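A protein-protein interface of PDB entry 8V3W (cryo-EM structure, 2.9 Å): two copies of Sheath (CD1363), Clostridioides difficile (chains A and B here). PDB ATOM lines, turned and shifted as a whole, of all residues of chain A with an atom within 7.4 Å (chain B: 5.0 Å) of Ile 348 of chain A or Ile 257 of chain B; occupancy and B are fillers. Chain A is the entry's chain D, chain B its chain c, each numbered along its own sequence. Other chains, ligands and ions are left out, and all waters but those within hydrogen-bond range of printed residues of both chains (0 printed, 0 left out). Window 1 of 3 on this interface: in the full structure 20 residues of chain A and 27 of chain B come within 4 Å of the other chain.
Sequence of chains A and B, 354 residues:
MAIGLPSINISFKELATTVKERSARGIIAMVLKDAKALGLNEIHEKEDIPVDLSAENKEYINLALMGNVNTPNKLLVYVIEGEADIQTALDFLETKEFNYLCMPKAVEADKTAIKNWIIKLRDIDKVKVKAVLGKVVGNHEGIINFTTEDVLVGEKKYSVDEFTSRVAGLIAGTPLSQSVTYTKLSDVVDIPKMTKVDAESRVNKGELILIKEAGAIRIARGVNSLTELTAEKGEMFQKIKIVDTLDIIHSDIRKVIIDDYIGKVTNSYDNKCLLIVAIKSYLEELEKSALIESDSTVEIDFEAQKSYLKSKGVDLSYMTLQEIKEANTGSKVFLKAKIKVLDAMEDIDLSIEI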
ATOM      1  N   MET A 345     -13.665  -7.984   1.561  1.00  0.00           N
ATOM      2  CA  MET A 345     -14.326  -9.102   2.222  1.00  0.00           C
ATOM      3  C   MET A 345     -15.065  -9.963   1.210  1.00  0.00           C
ATOM      4  O   MET A 345     -15.828  -9.452   0.387  1.00  0.00           O
ATOM      5  CB  MET A 345     -15.310  -8.599   3.274  1.00  0.00           C
ATOM      6  CG  MET A 345     -14.703  -7.846   4.426  1.00  0.00           C
ATOM      7  SD  MET A 345     -15.952  -7.504   5.678  1.00  0.00           S
ATOM      8  CE  MET A 345     -14.999  -6.562   6.851  1.00  0.00           C
ATOM      9  N   GLU A 346     -14.840 -11.275   1.271  1.00  0.00           N
ATOM     10  CA  GLU A 346     -15.545 -12.191   0.385  1.00  0.00           C
ATOM     11  C   GLU A 346     -15.999 -13.486   1.040  1.00  0.00           C
ATOM     12  O   GLU A 346     -16.811 -14.192   0.436  1.00  0.00           O
ATOM     13  CB  GLU A 346     -14.670 -12.517  -0.831  1.00  0.00           C
ATOM     14  CG  GLU A 346     -14.636 -11.397  -1.855  1.00  0.00           C
ATOM     15  CD  GLU A 346     -13.484 -11.515  -2.825  1.00  0.00           C
ATOM     16  OE1 GLU A 346     -12.708 -12.486  -2.718  1.00  0.00           O
ATOM     17  OE2 GLU A 346     -13.352 -10.634  -3.695  1.00  0.00           O
ATOM     18  N   ASP A 347     -15.518 -13.834   2.233  1.00  0.00           N
ATOM     19  CA  ASP A 347     -15.936 -15.046   2.923  1.00  0.00           C
ATOM     20  C   ASP A 347     -16.100 -14.748   4.403  1.00  0.00           C
ATOM     21  O   ASP A 347     -15.258 -14.075   5.000  1.00  0.00           O
ATOM     22  CB  ASP A 347     -14.924 -16.178   2.735  1.00  0.00           C
ATOM     23  CG  ASP A 347     -14.415 -16.273   1.316  1.00  0.00           C
ATOM     24  OD1 ASP A 347     -13.412 -15.607   0.998  1.00  0.00           O
ATOM     25  OD2 ASP A 347     -15.012 -17.023   0.520  1.00  0.00           O
ATOM     26  N   ILE A 348     -17.180 -15.252   4.996  1.00  0.00           N
ATOM     27  CA  ILE A 348     -17.504 -14.971   6.390  1.00  0.00           C
ATOM     28  C   ILE A 348     -17.962 -16.256   7.066  1.00  0.00           C
ATOM     29  O   ILE A 348     -18.770 -17.002   6.507  1.00  0.00           O
ATOM     30  CB  ILE A 348     -18.582 -13.878   6.513  1.00  0.00           C
ATOM     31  CG1 ILE A 348     -18.052 -12.555   5.962  1.00  0.00           C
ATOM     32  CG2 ILE A 348     -19.010 -13.705   7.953  1.00  0.00           C
ATOM     33  CD1 ILE A 348     -19.038 -11.428   6.019  1.00  0.00           C
ATOM     34  N   ASP A 349     -17.443 -16.513   8.264  1.00  0.00           N
ATOM     35  CA  ASP A 349     -17.865 -17.634   9.094  1.00  0.00           C
ATOM     36  C   ASP A 349     -18.461 -17.092  10.383  1.00  0.00           C
ATOM     37  O   ASP A 349     -17.815 -16.309  11.084  1.00  0.00           O
ATOM     38  CB  ASP A 349     -16.693 -18.560   9.415  1.00  0.00           C
ATOM     39  CG  ASP A 349     -16.299 -19.428   8.245  1.00  0.00           C
ATOM     40  OD1 ASP A 349     -16.707 -19.117   7.108  1.00  0.00           O
ATOM     41  OD2 ASP A 349     -15.578 -20.424   8.460  1.00  0.00           O
ATOM     42  N   LEU A 350     -19.683 -17.511  10.700  1.00  0.00           N
ATOM     43  CA  LEU A 350     -20.366 -17.085  11.917  1.00  0.00           C
ATOM     44  C   LEU A 350     -20.904 -18.317  12.628  1.00  0.00           C
ATOM     45  O   LEU A 350     -21.906 -18.895  12.200  1.00  0.00           O
ATOM     46  CB  LEU A 350     -21.493 -16.102  11.603  1.00  0.00           C
ATOM     47  CG  LEU A 350     -22.316 -15.590  12.787  1.00  0.00           C
ATOM     48  CD1 LEU A 350     -21.426 -15.146  13.927  1.00  0.00           C
ATOM     49  CD2 LEU A 350     -23.228 -14.464  12.358  1.00  0.00           C
ATOM     50  N   ILE B 253     -29.579 -12.497   8.798  1.00  0.00           N
ATOM     51  CA  ILE B 253     -28.160 -12.168   8.880  1.00  0.00           C
ATOM     52  C   ILE B 253     -27.506 -12.308   7.511  1.00  0.00           C
ATOM     53  O   ILE B 253     -26.664 -11.484   7.120  1.00  0.00           O
ATOM     54  CB  ILE B 253     -27.462 -13.031   9.945  1.00  0.00           C
ATOM     55  CG1 ILE B 253     -27.936 -12.625  11.338  1.00  0.00           C
ATOM     56  CG2 ILE B 253     -25.960 -12.868   9.857  1.00  0.00           C
ATOM     57  CD1 ILE B 253     -27.228 -13.339  12.452  1.00  0.00           C
ATOM     58  N   ARG B 254     -27.891 -13.338   6.752  1.00  0.00           N
ATOM     59  CA  ARG B 254     -27.338 -13.495   5.413  1.00  0.00           C
ATOM     60  C   ARG B 254     -27.692 -12.305   4.530  1.00  0.00           C
ATOM     61  O   ARG B 254     -26.846 -11.807   3.775  1.00  0.00           O
ATOM     62  CB  ARG B 254     -27.841 -14.797   4.792  1.00  0.00           C
ATOM     63  CG  ARG B 254     -26.750 -15.651   4.197  1.00  0.00           C
ATOM     64  CD  ARG B 254     -27.318 -16.873   3.510  1.00  0.00           C
ATOM     65  NE  ARG B 254     -26.448 -17.331   2.435  1.00  0.00           N
ATOM     66  CZ  ARG B 254     -26.660 -17.084   1.151  1.00  0.00           C
ATOM     67  NH1 ARG B 254     -27.723 -16.413   0.742  1.00  0.00           N
ATOM     68  NH2 ARG B 254     -25.781 -17.522   0.254  1.00  0.00           N
ATOM     69  N   LYS B 255     -28.936 -11.832   4.618  1.00  0.00           N
ATOM     70  CA  LYS B 255     -29.347 -10.677   3.829  1.00  0.00           C
ATOM     71  C   LYS B 255     -28.517  -9.451   4.174  1.00  0.00           C
ATOM     72  O   LYS B 255     -28.052  -8.733   3.283  1.00  0.00           O
ATOM     73  CB  LYS B 255     -30.829 -10.389   4.052  1.00  0.00           C
ATOM     74  CG  LYS B 255     -31.324  -9.180   3.294  1.00  0.00           C
ATOM     75  CD  LYS B 255     -32.827  -9.040   3.388  1.00  0.00           C
ATOM     76  CE  LYS B 255     -33.348  -8.102   2.320  1.00  0.00           C
ATOM     77  NZ  LYS B 255     -32.708  -6.765   2.419  1.00  0.00           N
ATOM     78  N   VAL B 256     -28.318  -9.195   5.469  1.00  0.00           N
ATOM     79  CA  VAL B 256     -27.549  -8.019   5.877  1.00  0.00           C
ATOM     80  C   VAL B 256     -26.127  -8.100   5.336  1.00  0.00           C
ATOM     81  O   VAL B 256     -25.616  -7.151   4.718  1.00  0.00           O
ATOM     82  CB  VAL B 256     -27.563  -7.872   7.408  1.00  0.00           C
ATOM     83  CG1 VAL B 256     -26.378  -7.053   7.876  1.00  0.00           C
ATOM     84  CG2 VAL B 256     -28.861  -7.240   7.863  1.00  0.00           C
ATOM     85  N   ILE B 257     -25.478  -9.252   5.530  1.00  0.00           N
ATOM     86  CA  ILE B 257     -24.087  -9.400   5.109  1.00  0.00           C
ATOM     87  C   ILE B 257     -23.961  -9.210   3.603  1.00  0.00           C
ATOM     88  O   ILE B 257     -23.084  -8.482   3.126  1.00  0.00           O
ATOM     89  CB  ILE B 257     -23.533 -10.767   5.548  1.00  0.00           C
ATOM     90  CG1 ILE B 257     -23.092 -10.727   7.007  1.00  0.00           C
ATOM     91  CG2 ILE B 257     -22.375 -11.178   4.667  1.00  0.00           C
ATOM     92  CD1 ILE B 257     -22.712 -12.081   7.547  1.00  0.00           C
ATOM     93  N   ILE B 258     -24.843  -9.850   2.831  1.00  0.00           N
ATOM     94  CA  ILE B 258     -24.734  -9.771   1.377  1.00  0.00           C
ATOM     95  C   ILE B 258     -25.022  -8.357   0.891  1.00  0.00           C
ATOM     96  O   ILE B 258     -24.351  -7.850  -0.014  1.00  0.00           O
ATOM     97  CB  ILE B 258     -25.664 -10.803   0.716  1.00  0.00           C
ATOM     98  CG1 ILE B 258     -25.113 -12.212   0.909  1.00  0.00           C
ATOM     99  CG2 ILE B 258     -25.830 -10.513  -0.765  1.00  0.00           C
ATOM    100  CD1 ILE B 258     -25.945 -13.277   0.251  1.00  0.00           C
ATOM    101  N   ASP B 259     -26.013  -7.691   1.485  1.00  0.00           N
ATOM    102  CA  ASP B 259     -26.393  -6.366   1.011  1.00  0.00           C
ATOM    103  C   ASP B 259     -25.306  -5.334   1.273  1.00  0.00           C
ATOM    104  O   ASP B 259     -25.043  -4.480   0.419  1.00  0.00           O
ATOM    105  CB  ASP B 259     -27.701  -5.931   1.668  1.00  0.00           C
ATOM    106  CG  ASP B 259     -28.917  -6.331   0.866  1.00  0.00           C
ATOM    107  OD1 ASP B 259     -28.746  -6.947  -0.205  1.00  0.00           O
ATOM    108  OD2 ASP B 259     -30.046  -6.038   1.313  1.00  0.00           O
ATOM    109  N   ASP B 260     -24.666  -5.377   2.445  1.00  0.00           N
ATOM    110  CA  ASP B 260     -23.863  -4.232   2.851  1.00  0.00           C
ATOM    111  C   ASP B 260     -22.353  -4.438   2.855  1.00  0.00           C
ATOM    112  O   ASP B 260     -21.626  -3.443   2.907  1.00  0.00           O
ATOM    113  CB  ASP B 260     -24.292  -3.757   4.247  1.00  0.00           C
ATOM    114  CG  ASP B 260     -25.679  -3.156   4.254  1.00  0.00           C
ATOM    115  OD1 ASP B 260     -25.914  -2.204   3.484  1.00  0.00           O
ATOM    116  OD2 ASP B 260     -26.539  -3.639   5.018  1.00  0.00           O
ATOM    117  N   TYR B 261     -21.850  -5.673   2.796  1.00  0.00           N
ATOM    118  CA  TYR B 261     -20.423  -5.845   3.059  1.00  0.00           C
ATOM    119  C   TYR B 261     -19.666  -6.668   2.021  1.00  0.00           C
ATOM    120  O   TYR B 261     -18.478  -6.423   1.796  1.00  0.00           O
ATOM    121  CB  TYR B 261     -20.231  -6.468   4.442  1.00  0.00           C
ATOM    122  CG  TYR B 261     -20.623  -5.538   5.562  1.00  0.00           C
ATOM    123  CD1 TYR B 261     -21.923  -5.509   6.035  1.00  0.00           C
ATOM    124  CD2 TYR B 261     -19.700  -4.679   6.135  1.00  0.00           C
ATOM    125  CE1 TYR B 261     -22.293  -4.662   7.045  1.00  0.00           C
ATOM    126  CE2 TYR B 261     -20.061  -3.827   7.151  1.00  0.00           C
ATOM    127  CZ  TYR B 261     -21.360  -3.822   7.601  1.00  0.00           C
ATOM    128  OH  TYR B 261     -21.734  -2.974   8.613  1.00  0.00           O
ATOM    129  N   ILE B 262     -20.317  -7.639   1.387  1.00  0.00           N
ATOM    130  CA  ILE B 262     -19.597  -8.567   0.520  1.00  0.00           C
ATOM    131  C   ILE B 262     -19.123  -7.834  -0.728  1.00  0.00           C
ATOM    132  O   ILE B 262     -19.930  -7.350  -1.528  1.00  0.00           O
ATOM    133  CB  ILE B 262     -20.470  -9.772   0.155  1.00  0.00           C
ATOM    134  CG1 ILE B 262     -20.636 -10.694   1.361  1.00  0.00           C
ATOM    135  CG2 ILE B 262     -19.848 -10.544  -0.986  1.00  0.00           C
ATOM    136  CD1 ILE B 262     -19.350 -10.964   2.099  1.00  0.00           C
ATOM    137  N   LEU B 275     -18.918  -4.539  11.273  1.00  0.00           N
ATOM    138  CA  LEU B 275     -19.816  -5.661  11.008  1.00  0.00           C
ATOM    139  C   LEU B 275     -20.354  -6.261  12.303  1.00  0.00           C
ATOM    140  O   LEU B 275     -21.539  -6.614  12.394  1.00  0.00           O
ATOM    141  CB  LEU B 275     -19.088  -6.722  10.186  1.00  0.00           C
ATOM    142  CG  LEU B 275     -19.920  -7.802   9.499  1.00  0.00           C
ATOM    143  CD1 LEU B 275     -19.282  -8.215   8.198  1.00  0.00           C
ATOM    144  CD2 LEU B 275     -20.046  -8.996  10.393  1.00  0.00           C
ATOM    145  N   ILE B 279     -24.354  -6.684  13.406  1.00  0.00           N
ATOM    146  CA  ILE B 279     -24.988  -7.949  13.781  1.00  0.00           C
ATOM    147  C   ILE B 279     -25.572  -7.863  15.187  1.00  0.00           C
ATOM    148  O   ILE B 279     -26.681  -8.350  15.449  1.00  0.00           O
ATOM    149  CB  ILE B 279     -23.987  -9.113  13.649  1.00  0.00           C
ATOM    150  CG1 ILE B 279     -23.650  -9.364  12.184  1.00  0.00           C
ATOM    151  CG2 ILE B 279     -24.558 -10.378  14.251  1.00  0.00           C
ATOM    152  CD1 ILE B 279     -22.807 -10.587  11.965  1.00  0.00           C
ATOM    153  N   VAL B 333     -13.277 -13.747   7.313  1.00  0.00           N
ATOM    154  CA  VAL B 333     -13.695 -13.205   8.602  1.00  0.00           C
ATOM    155  C   VAL B 333     -14.226 -14.346   9.457  1.00  0.00           C
ATOM    156  O   VAL B 333     -14.951 -15.215   8.964  1.00  0.00           O
ATOM    157  CB  VAL B 333     -14.766 -12.106   8.438  1.00  0.00           C
ATOM    158  CG1 VAL B 333     -15.129 -11.500   9.779  1.00  0.00           C
ATOM    159  CG2 VAL B 333     -14.283 -11.029   7.492  1.00  0.00           C
ATOM    160  N   LEU B 335     -16.219 -15.132  13.148  1.00  0.00           N
ATOM    161  CA  LEU B 335     -16.997 -14.578  14.245  1.00  0.00           C
ATOM    162  C   LEU B 335     -17.677 -15.700  15.015  1.00  0.00           C
ATOM    163  O   LEU B 335     -17.768 -16.836  14.549  1.00  0.00           O
ATOM    164  CB  LEU B 335     -18.057 -13.587  13.754  1.00  0.00           C
ATOM    165  CG  LEU B 335     -17.670 -12.500  12.754  1.00  0.00           C
ATOM    166  CD1 LEU B 335     -18.919 -11.812  12.266  1.00  0.00           C
ATOM    167  CD2 LEU B 335     -16.721 -11.495  13.375  1.00  0.00           C
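Along chain B the printed residues that touch a printed residue of chain A span positions 257 to 335. Hydrophobic or aromatic side chains of chain A that line the printed part of chain B: Ile 348 and Leu 350. Among the printed residues, no Asp or Glu carboxylate lies within 4 Å of a Lys or Arg side-chain nitrogen of the other chain.
O of Asp 347 of chain A is in hydrogen-bond range of N of Val 333 of chain B (3.1 Å). The backbone NH of Asp 349 of chain A sits at hydrogen-bond distance from the backbone carbonyl oxygen of Val 333 of chain B, at 2.9 Å. The backbone carbonyl oxygen of Asp 349 of chain A lies within hydrogen-bond range of the backbone NH of Leu 335 of chain B, 2.9 Å away.
N of Ile 262 of chain B is in hydrogen-bond range of O of Ile 257 of chain B.
Among the printed residues, pairs that only touch across the chains: Met 345 of chain A with Ile 262 of chain B (3.8 Å), Ile 348 of chain A with Ile 257 of chain B (3.6 Å), Ile 348 of chain A with Ile 262 of chain B (3.96 Å), Ile 348 of chain A with Leu 275 of chain B (3.9 Å), Ile 348 of chain A with Val 333 of chain B (3.6 Å), Leu 350 of chain A with Ile 279 of chain B (3.9 Å) and Leu 350 of chain A with Leu 335 of chain B (3.7 Å).
No position is printed for both chains.
Ile 348 of chain A touches just these residues of chain B: Ile 257 (3.6 Å), Ile 262 (3.96 Å), Leu 275 (3.9 Å) and Val 333 (3.6 Å). Of the printed residues of chain B, Leu 350 of chain A touches Ile 279 (3.9 Å) and Leu 335 (3.7 Å). Val 256 of chain B touches none of the printed residues of chain A. Ile 257 of chain B touches just one residue of chain A: Ile 348. Of the printed residues of chain A, Leu 275 of chain B touches Ile 348 (3.9 Å). The nearest residue of chain A that does not touch Ile 257 of chain B is Leu 350 of chain A (5.4 Å).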
